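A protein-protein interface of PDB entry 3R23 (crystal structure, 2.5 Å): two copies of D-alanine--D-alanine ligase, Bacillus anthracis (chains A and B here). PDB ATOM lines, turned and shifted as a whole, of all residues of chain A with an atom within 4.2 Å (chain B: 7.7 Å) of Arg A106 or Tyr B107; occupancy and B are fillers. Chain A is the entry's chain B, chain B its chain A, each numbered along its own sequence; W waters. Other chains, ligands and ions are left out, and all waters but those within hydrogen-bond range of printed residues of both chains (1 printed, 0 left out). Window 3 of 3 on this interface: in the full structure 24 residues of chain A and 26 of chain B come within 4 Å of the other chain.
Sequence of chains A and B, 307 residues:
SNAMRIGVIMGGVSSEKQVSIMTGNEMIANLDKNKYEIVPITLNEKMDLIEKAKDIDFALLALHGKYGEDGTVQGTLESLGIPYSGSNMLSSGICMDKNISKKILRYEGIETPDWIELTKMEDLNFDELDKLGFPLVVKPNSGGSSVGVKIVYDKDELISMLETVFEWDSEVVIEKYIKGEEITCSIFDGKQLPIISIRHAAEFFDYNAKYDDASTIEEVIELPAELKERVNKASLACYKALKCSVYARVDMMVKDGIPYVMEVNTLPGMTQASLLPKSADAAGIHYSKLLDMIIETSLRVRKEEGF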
ATOM      1  N   LYS A 102     -23.282  12.791  -0.691  1.00  0.00           N
ATOM      2  CA  LYS A 102     -23.933  13.984  -0.195  1.00  0.00           C
ATOM      3  C   LYS A 102     -23.379  14.361   1.183  1.00  0.00           C
ATOM      4  O   LYS A 102     -23.191  15.558   1.462  1.00  0.00           O
ATOM      5  CB  LYS A 102     -25.461  13.880  -0.277  1.00  0.00           C
ATOM      6  CG  LYS A 102     -25.955  14.179  -1.688  1.00  0.00           C
ATOM      7  CD  LYS A 102     -27.095  13.261  -2.135  1.00  0.00           C
ATOM      8  CE  LYS A 102     -28.427  13.613  -1.498  1.00  0.00           C
ATOM      9  NZ  LYS A 102     -28.866  15.009  -1.856  1.00  0.00           N
ATOM     10  N   LYS A 103     -23.053  13.342   1.991  1.00  0.00           N
ATOM     11  CA  LYS A 103     -22.466  13.539   3.320  1.00  0.00           C
ATOM     12  C   LYS A 103     -21.158  14.291   3.209  1.00  0.00           C
ATOM     13  O   LYS A 103     -20.972  15.297   3.855  1.00  0.00           O
ATOM     14  CB  LYS A 103     -22.275  12.216   4.050  1.00  0.00           C
ATOM     15  CG  LYS A 103     -23.557  11.653   4.647  1.00  0.00           C
ATOM     16  CD  LYS A 103     -23.502  10.138   4.842  1.00  0.00           C
ATOM     17  CE  LYS A 103     -23.955   9.776   6.241  1.00  0.00           C
ATOM     18  NZ  LYS A 103     -24.867   8.611   6.282  1.00  0.00           N
ATOM     19  N   ILE A 104     -20.269  13.836   2.349  1.00  0.00           N
ATOM     20  CA  ILE A 104     -19.038  14.566   2.115  1.00  0.00           C
ATOM     21  C   ILE A 104     -19.328  15.957   1.535  1.00  0.00           C
ATOM     22  O   ILE A 104     -18.573  16.884   1.773  1.00  0.00           O
ATOM     23  CB  ILE A 104     -18.094  13.794   1.187  1.00  0.00           C
ATOM     24  CG1 ILE A 104     -17.815  12.392   1.736  1.00  0.00           C
ATOM     25  CG2 ILE A 104     -16.802  14.527   1.008  1.00  0.00           C
ATOM     26  CD1 ILE A 104     -17.056  11.501   0.752  1.00  0.00           C
ATOM     27  N   LEU A 105     -20.416  16.114   0.778  1.00  0.00           N
ATOM     28  CA  LEU A 105     -20.740  17.429   0.199  1.00  0.00           C
ATOM     29  C   LEU A 105     -21.269  18.409   1.246  1.00  0.00           C
ATOM     30  O   LEU A 105     -20.755  19.519   1.372  1.00  0.00           O
ATOM     31  CB  LEU A 105     -21.736  17.318  -0.950  1.00  0.00           C
ATOM     32  CG  LEU A 105     -21.182  16.786  -2.273  1.00  0.00           C
ATOM     33  CD1 LEU A 105     -22.292  16.504  -3.263  1.00  0.00           C
ATOM     34  CD2 LEU A 105     -20.129  17.711  -2.872  1.00  0.00           C
ATOM     35  N   ARG A 106     -22.268  17.992   2.017  1.00  0.00           N
ATOM     36  CA  ARG A 106     -22.723  18.808   3.143  1.00  0.00           C
ATOM     37  C   ARG A 106     -21.641  19.163   4.195  1.00  0.00           C
ATOM     38  O   ARG A 106     -21.645  20.272   4.751  1.00  0.00           O
ATOM     39  CB  ARG A 106     -23.919  18.172   3.829  1.00  0.00           C
ATOM     40  CG  ARG A 106     -24.406  18.977   5.012  1.00  0.00           C
ATOM     41  CD  ARG A 106     -25.900  18.775   5.181  1.00  0.00           C
ATOM     42  NE  ARG A 106     -26.594  19.048   3.926  1.00  0.00           N
ATOM     43  CZ  ARG A 106     -27.889  18.824   3.724  1.00  0.00           C
ATOM     44  NH1 ARG A 106     -28.640  18.300   4.696  1.00  0.00           N
ATOM     45  NH2 ARG A 106     -28.432  19.113   2.546  1.00  0.00           N
ATOM     46  N   TYR A 107     -20.718  18.250   4.486  1.00  0.00           N
ATOM     47  CA  TYR A 107     -19.668  18.617   5.421  1.00  0.00           C
ATOM     48  C   TYR A 107     -18.887  19.840   4.889  1.00  0.00           C
ATOM     49  O   TYR A 107     -18.426  20.674   5.667  1.00  0.00           O
ATOM     50  CB  TYR A 107     -18.750  17.433   5.791  1.00  0.00           C
ATOM     51  CG  TYR A 107     -17.518  17.857   6.573  1.00  0.00           C
ATOM     52  CD1 TYR A 107     -17.534  17.911   7.954  1.00  0.00           C
ATOM     53  CD2 TYR A 107     -16.347  18.236   5.924  1.00  0.00           C
ATOM     54  CE1 TYR A 107     -16.410  18.330   8.689  1.00  0.00           C
ATOM     55  CE2 TYR A 107     -15.214  18.645   6.640  1.00  0.00           C
ATOM     56  CZ  TYR A 107     -15.252  18.693   8.025  1.00  0.00           C
ATOM     57  OH  TYR A 107     -14.128  19.090   8.752  1.00  0.00           O
ATOM     58  N   GLU A 108     -18.752  19.956   3.572  1.00  0.00           N
ATOM     59  CA  GLU A 108     -18.124  21.148   2.986  1.00  0.00           C
ATOM     60  C   GLU A 108     -19.100  22.350   2.822  1.00  0.00           C
ATOM     61  O   GLU A 108     -18.696  23.452   2.422  1.00  0.00           O
ATOM     62  CB  GLU A 108     -17.515  20.799   1.632  1.00  0.00           C
ATOM     63  CG  GLU A 108     -16.042  21.066   1.533  1.00  0.00           C
ATOM     64  CD  GLU A 108     -15.217  19.868   1.955  1.00  0.00           C
ATOM     65  OE1 GLU A 108     -14.231  19.551   1.247  1.00  0.00           O
ATOM     66  OE2 GLU A 108     -15.553  19.249   2.993  1.00  0.00           O
ATOM     67  N   GLY A 109     -20.380  22.108   3.116  1.00  0.00           N
ATOM     68  CA  GLY A 109     -21.420  23.107   2.998  1.00  0.00           C
ATOM     69  C   GLY A 109     -21.702  23.455   1.557  1.00  0.00           C
ATOM     70  O   GLY A 109     -22.059  24.590   1.236  1.00  0.00           O
ATOM     71  N   THR A 112     -26.591  20.816  -1.615  1.00  0.00           N
ATOM     72  CA  THR A 112     -27.265  19.674  -2.199  1.00  0.00           C
ATOM     73  C   THR A 112     -28.567  19.447  -1.420  1.00  0.00           C
ATOM     74  O   THR A 112     -28.582  19.558  -0.201  1.00  0.00           O
ATOM     75  CB  THR A 112     -26.318  18.418  -2.175  1.00  0.00           C
ATOM     76  OG1 THR A 112     -26.996  17.256  -2.675  1.00  0.00           O
ATOM     77  CG2 THR A 112     -25.839  18.149  -0.771  1.00  0.00           C
ATOM     78  N   PRO A 113     -29.641  19.035  -2.106  1.00  0.00           N
ATOM     79  CA  PRO A 113     -30.928  18.861  -1.435  1.00  0.00           C
ATOM     80  C   PRO A 113     -30.844  18.018  -0.166  1.00  0.00           C
ATOM     81  O   PRO A 113     -30.188  16.980  -0.153  1.00  0.00           O
ATOM     82  CB  PRO A 113     -31.744  18.092  -2.473  1.00  0.00           C
ATOM     83  CG  PRO A 113     -31.173  18.485  -3.761  1.00  0.00           C
ATOM     84  CD  PRO A 113     -29.717  18.693  -3.537  1.00  0.00           C
ATOM     85  N   ASP A 114     -31.558  18.431   0.873  1.00  0.00           N
ATOM     86  CA  ASP A 114     -31.628  17.658   2.095  1.00  0.00           C
ATOM     87  C   ASP A 114     -32.191  16.292   1.740  1.00  0.00           C
ATOM     88  O   ASP A 114     -32.896  16.148   0.749  1.00  0.00           O
ATOM     89  CB  ASP A 114     -32.533  18.357   3.098  1.00  0.00           C
ATOM     90  CG  ASP A 114     -31.940  19.669   3.596  1.00  0.00           C
ATOM     91  OD1 ASP A 114     -30.729  19.684   3.928  1.00  0.00           O
ATOM     92  OD2 ASP A 114     -32.680  20.683   3.647  1.00  0.00           O
ATOM     93  N   TRP A 115     -31.851  15.267   2.505  1.00  0.00           N
ATOM     94  CA  TRP A 115     -32.292  13.950   2.088  1.00  0.00           C
ATOM     95  C   TRP A 115     -32.396  12.941   3.213  1.00  0.00           C
ATOM     96  O   TRP A 115     -32.195  13.256   4.383  1.00  0.00           O
ATOM     97  CB  TRP A 115     -31.364  13.413   0.996  1.00  0.00           C
ATOM     98  CG  TRP A 115     -30.082  12.836   1.526  1.00  0.00           C
ATOM     99  CD1 TRP A 115     -29.774  11.502   1.669  1.00  0.00           C
ATOM    100  CD2 TRP A 115     -28.937  13.561   2.002  1.00  0.00           C
ATOM    101  NE1 TRP A 115     -28.517  11.366   2.194  1.00  0.00           N
ATOM    102  CE2 TRP A 115     -27.980  12.610   2.407  1.00  0.00           C
ATOM    103  CE3 TRP A 115     -28.634  14.920   2.120  1.00  0.00           C
ATOM    104  CZ2 TRP A 115     -26.726  12.978   2.921  1.00  0.00           C
ATOM    105  CZ3 TRP A 115     -27.388  15.286   2.632  1.00  0.00           C
ATOM    106  CH2 TRP A 115     -26.450  14.313   3.024  1.00  0.00           C
ATOM    107  N   SER B 101     -13.256   9.437   6.087  1.00  0.00           N
ATOM    108  CA  SER B 101     -13.875   8.824   7.278  1.00  0.00           C
ATOM    109  C   SER B 101     -14.335   9.856   8.320  1.00  0.00           C
ATOM    110  O   SER B 101     -15.415   9.731   8.885  1.00  0.00           O
ATOM    111  CB  SER B 101     -12.931   7.823   7.976  1.00  0.00           C
ATOM    112  OG  SER B 101     -12.883   6.601   7.292  1.00  0.00           O
ATOM    113  N   LYS B 102     -13.491  10.839   8.604  1.00  0.00           N
ATOM    114  CA  LYS B 102     -13.817  11.822   9.625  1.00  0.00           C
ATOM    115  C   LYS B 102     -14.951  12.711   9.149  1.00  0.00           C
ATOM    116  O   LYS B 102     -15.831  13.057   9.926  1.00  0.00           O
ATOM    117  CB  LYS B 102     -12.579  12.622  10.078  1.00  0.00           C
ATOM    118  CG  LYS B 102     -11.664  11.779  10.996  1.00  0.00           C
ATOM    119  CD  LYS B 102     -10.275  12.371  11.197  1.00  0.00           C
ATOM    120  CE  LYS B 102     -10.275  13.483  12.211  1.00  0.00           C
ATOM    121  NZ  LYS B 102     -10.815  13.041  13.528  1.00  0.00           N
ATOM    122  N   LYS B 103     -14.935  13.061   7.869  1.00  0.00           N
ATOM    123  CA  LYS B 103     -16.023  13.846   7.301  1.00  0.00           C
ATOM    124  C   LYS B 103     -17.367  13.131   7.457  1.00  0.00           C
ATOM    125  O   LYS B 103     -18.358  13.778   7.816  1.00  0.00           O
ATOM    126  CB  LYS B 103     -15.753  14.167   5.829  1.00  0.00           C
ATOM    127  CG  LYS B 103     -14.794  15.308   5.634  1.00  0.00           C
ATOM    128  CD  LYS B 103     -14.243  15.353   4.226  1.00  0.00           C
ATOM    129  CE  LYS B 103     -13.355  16.578   4.086  1.00  0.00           C
ATOM    130  NZ  LYS B 103     -13.072  16.988   2.678  1.00  0.00           N
ATOM    131  N   ILE B 104     -17.401  11.810   7.208  1.00  0.00           N
ATOM    132  CA  ILE B 104     -18.656  11.049   7.299  1.00  0.00           C
ATOM    133  C   ILE B 104     -19.146  10.784   8.714  1.00  0.00           C
ATOM    134  O   ILE B 104     -20.359  10.791   8.954  1.00  0.00           O
ATOM    135  CB  ILE B 104     -18.591   9.702   6.594  1.00  0.00           C
ATOM    136  CG1 ILE B 104     -18.368   9.877   5.101  1.00  0.00           C
ATOM    137  CG2 ILE B 104     -19.868   8.915   6.846  1.00  0.00           C
ATOM    138  CD1 ILE B 104     -17.700   8.709   4.503  1.00  0.00           C
ATOM    139  N   LEU B 105     -18.229  10.517   9.645  1.00  0.00           N
ATOM    140  CA  LEU B 105     -18.607  10.360  11.055  1.00  0.00           C
ATOM    141  C   LEU B 105     -19.070  11.692  11.651  1.00  0.00           C
ATOM    142  O   LEU B 105     -19.991  11.758  12.456  1.00  0.00           O
ATOM    143  CB  LEU B 105     -17.417   9.876  11.872  1.00  0.00           C
ATOM    144  CG  LEU B 105     -16.852   8.503  11.582  1.00  0.00           C
ATOM    145  CD1 LEU B 105     -15.518   8.467  12.274  1.00  0.00           C
ATOM    146  CD2 LEU B 105     -17.785   7.402  12.079  1.00  0.00           C
ATOM    147  N   ARG B 106     -18.368  12.752  11.288  1.00  0.00           N
ATOM    148  CA  ARG B 106     -18.670  14.082  11.775  1.00  0.00           C
ATOM    149  C   ARG B 106     -20.104  14.417  11.316  1.00  0.00           C
ATOM    150  O   ARG B 106     -20.909  14.867  12.111  1.00  0.00           O
ATOM    151  CB  ARG B 106     -17.575  15.059  11.291  1.00  0.00           C
ATOM    152  CG  ARG B 106     -17.692  16.562  11.622  1.00  0.00           C
ATOM    153  CD  ARG B 106     -17.660  16.937  13.126  1.00  0.00           C
ATOM    154  NE  ARG B 106     -16.394  16.810  13.874  1.00  0.00           N
ATOM    155  CZ  ARG B 106     -15.330  17.607  13.756  1.00  0.00           C
ATOM    156  NH1 ARG B 106     -15.301  18.589  12.859  1.00  0.00           N
ATOM    157  NH2 ARG B 106     -14.264  17.402  14.524  1.00  0.00           N
ATOM    158  N   TYR B 107     -20.455  14.111  10.072  1.00  0.00           N
ATOM    159  CA  TYR B 107     -21.798  14.445   9.577  1.00  0.00           C
ATOM    160  C   TYR B 107     -22.897  13.906  10.451  1.00  0.00           C
ATOM    161  O   TYR B 107     -23.993  14.444  10.467  1.00  0.00           O
ATOM    162  CB  TYR B 107     -22.029  13.946   8.145  1.00  0.00           C
ATOM    163  CG  TYR B 107     -23.476  14.010   7.691  1.00  0.00           C
ATOM    164  CD1 TYR B 107     -23.962  15.127   7.045  1.00  0.00           C
ATOM    165  CD2 TYR B 107     -24.346  12.954   7.894  1.00  0.00           C
ATOM    166  CE1 TYR B 107     -25.279  15.212   6.616  1.00  0.00           C
ATOM    167  CE2 TYR B 107     -25.686  13.026   7.478  1.00  0.00           C
ATOM    168  CZ  TYR B 107     -26.139  14.171   6.841  1.00  0.00           C
ATOM    169  OH  TYR B 107     -27.439  14.281   6.401  1.00  0.00           O
ATOM    170  N   GLU B 108     -22.615  12.822  11.148  1.00  0.00           N
ATOM    171  CA  GLU B 108     -23.590  12.151  12.009  1.00  0.00           C
ATOM    172  C   GLU B 108     -23.496  12.663  13.428  1.00  0.00           C
ATOM    173  O   GLU B 108     -24.266  12.241  14.297  1.00  0.00           O
ATOM    174  CB  GLU B 108     -23.272  10.664  12.081  1.00  0.00           C
ATOM    175  CG  GLU B 108     -22.978  10.041  10.761  1.00  0.00           C
ATOM    176  CD  GLU B 108     -24.151   9.272  10.304  1.00  0.00           C
ATOM    177  OE1 GLU B 108     -24.657   8.511  11.159  1.00  0.00           O
ATOM    178  OE2 GLU B 108     -24.577   9.445   9.131  1.00  0.00           O
ATOM    179  N   GLY B 109     -22.514  13.522  13.667  1.00  0.00           N
ATOM    180  CA  GLY B 109     -22.247  14.010  15.007  1.00  0.00           C
ATOM    181  C   GLY B 109     -21.671  12.975  15.950  1.00  0.00           C
ATOM    182  O   GLY B 109     -21.987  12.963  17.138  1.00  0.00           O
ATOM    183  N   ILE B 110     -20.845  12.091  15.397  1.00  0.00           N
ATOM    184  CA  ILE B 110     -20.134  11.085  16.162  1.00  0.00           C
ATOM    185  C   ILE B 110     -18.846  11.766  16.557  1.00  0.00           C
ATOM    186  O   ILE B 110     -18.158  12.289  15.705  1.00  0.00           O
ATOM    187  CB  ILE B 110     -19.874   9.812  15.296  1.00  0.00           C
ATOM    188  CG1 ILE B 110     -21.191   9.091  15.021  1.00  0.00           C
ATOM    189  CG2 ILE B 110     -18.888   8.832  15.959  1.00  0.00           C
ATOM    190  CD1 ILE B 110     -21.064   7.960  14.022  1.00  0.00           C
ATOM    191  N   THR B 112     -15.355  12.969  17.090  1.00  0.00           N
ATOM    192  CA  THR B 112     -14.042  12.703  16.572  1.00  0.00           C
ATOM    193  C   THR B 112     -13.297  14.019  16.697  1.00  0.00           C
ATOM    194  O   THR B 112     -13.902  15.072  16.609  1.00  0.00           O
ATOM    195  CB  THR B 112     -14.128  12.210  15.109  1.00  0.00           C
ATOM    196  OG1 THR B 112     -12.883  11.598  14.727  1.00  0.00           O
ATOM    197  CG2 THR B 112     -14.494  13.368  14.141  1.00  0.00           C
ATOM    198  N   TRP B 115      -9.649  18.355  12.884  1.00  0.00           N
ATOM    199  CA  TRP B 115      -8.516  17.957  12.091  1.00  0.00           C
ATOM    200  C   TRP B 115      -8.433  18.872  10.894  1.00  0.00           C
ATOM    201  O   TRP B 115      -9.401  19.544  10.542  1.00  0.00           O
ATOM    202  CB  TRP B 115      -8.658  16.480  11.648  1.00  0.00           C
ATOM    203  CG  TRP B 115      -9.527  16.277  10.473  1.00  0.00           C
ATOM    204  CD1 TRP B 115      -9.122  16.130   9.173  1.00  0.00           C
ATOM    205  CD2 TRP B 115     -10.962  16.213  10.457  1.00  0.00           C
ATOM    206  NE1 TRP B 115     -10.209  15.961   8.357  1.00  0.00           N
ATOM    207  CE2 TRP B 115     -11.352  16.009   9.113  1.00  0.00           C
ATOM    208  CE3 TRP B 115     -11.951  16.292  11.447  1.00  0.00           C
ATOM    209  CZ2 TRP B 115     -12.695  15.905   8.725  1.00  0.00           C
ATOM    210  CZ3 TRP B 115     -13.290  16.178  11.062  1.00  0.00           C
ATOM    211  CH2 TRP B 115     -13.649  15.991   9.709  1.00  0.00           C
HETATM  212  O   HOH W   1     -11.648  19.211   8.346  1.00  0.00           O
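The side-chain carboxylate (OE1) of Glu A108 lies within salt-bridge range of the side-chain amino group (NZ) of Lys B103, at 3.2 Å. OE2 of Glu B108 lies within salt-bridge range of NZ of Lys A103, 3.0 Å away.
O of Thr B112 is in hydrogen-bond range of NH2 of Arg B106 (3.1 Å). NH2 of Arg A106 lies within hydrogen-bond range of O of Thr A112, at 2.8 Å. NH1 of Arg A106 lies within salt-bridge range of OD1 of Asp A114, 2.6 Å away.
Among the printed residues, merely in contact across the chains: Tyr A107 with Trp B115 (3.3 Å), Tyr A107 with Lys B103 (3.3 Å), Trp A115 with Tyr B107 (3.5 Å), Lys A103 with Tyr B107 (3.6 Å), Tyr A107 with Arg B106 (3.7 Å) and Arg A106 with Tyr B107 (3.9 Å).
Arg A106 touches one residue of chain B. Of the printed residues of chain A, Lys B103 touches Tyr A107 and Glu A108. Printed residues of chain A within 4 Å of Glu B108: Lys A103 (3.0 Å). Of the printed residues of chain B, Lys A103 touches Tyr B107 (3.6 Å) and Glu B108 (3.0 Å). Printed residues of chain A within 4 Å of Arg B106: Tyr A107 (3.7 Å). Of the printed residues of chain B, Tyr A107 touches Lys B103 (3.3 Å), Arg B106 (3.7 Å) and Trp B115 (3.3 Å). The nearest residue of chain B that does not touch Arg A106 is Lys B103 (7.3 Å). The nearest printed residue of chain A that does not touch Tyr B107 is Tyr A107 (5.2 Å).
Of the 12 printed residues of chain B, 5 touch a printed residue of chain A. Hydrophobic or aromatic side chains of chain B within 4 Å of the printed part of chain A: Tyr B107 and Trp B115. Of the 12 printed residues of chain A, 5 touch a printed residue of chain B. Printed residues of chain A that touch a printed residue of chain B: Lys A103, Arg A106, Tyr A107, Glu A108 and Trp A115. Among the printed residues, 8 pairs touch across the chains. Among the printed residues, Asp or Glu carboxylates within 4 Å of a Lys or Arg side-chain nitrogen of the other chain: Lys A103 with Glu B108 and Glu A108 with Lys B103.
Lys A103 touches Tyr B107, and with the chains exchanged Tyr A107 touches Lys B103. Lys A103 touches Glu B108, and with the chains exchanged Glu A108 touches Lys B103. Arg A106 touches Tyr B107, and with the chains exchanged Tyr A107 touches Arg B106. Tyr A107 touches Trp B115, and with the chains exchanged Trp A115 touches Tyr B107. Positions printed for both chains: 102, 103, 104, 105, 106, 107, 108, 109, 112 and 115. Of the 8 pairs that touch across the chains among the printed residues, 8 have their exchanged pair printed and touching as well.
Water W1 lies within hydrogen-bond range of OH of Tyr A107 (2.5 Å) and O of Trp B115 (3.2 Å).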
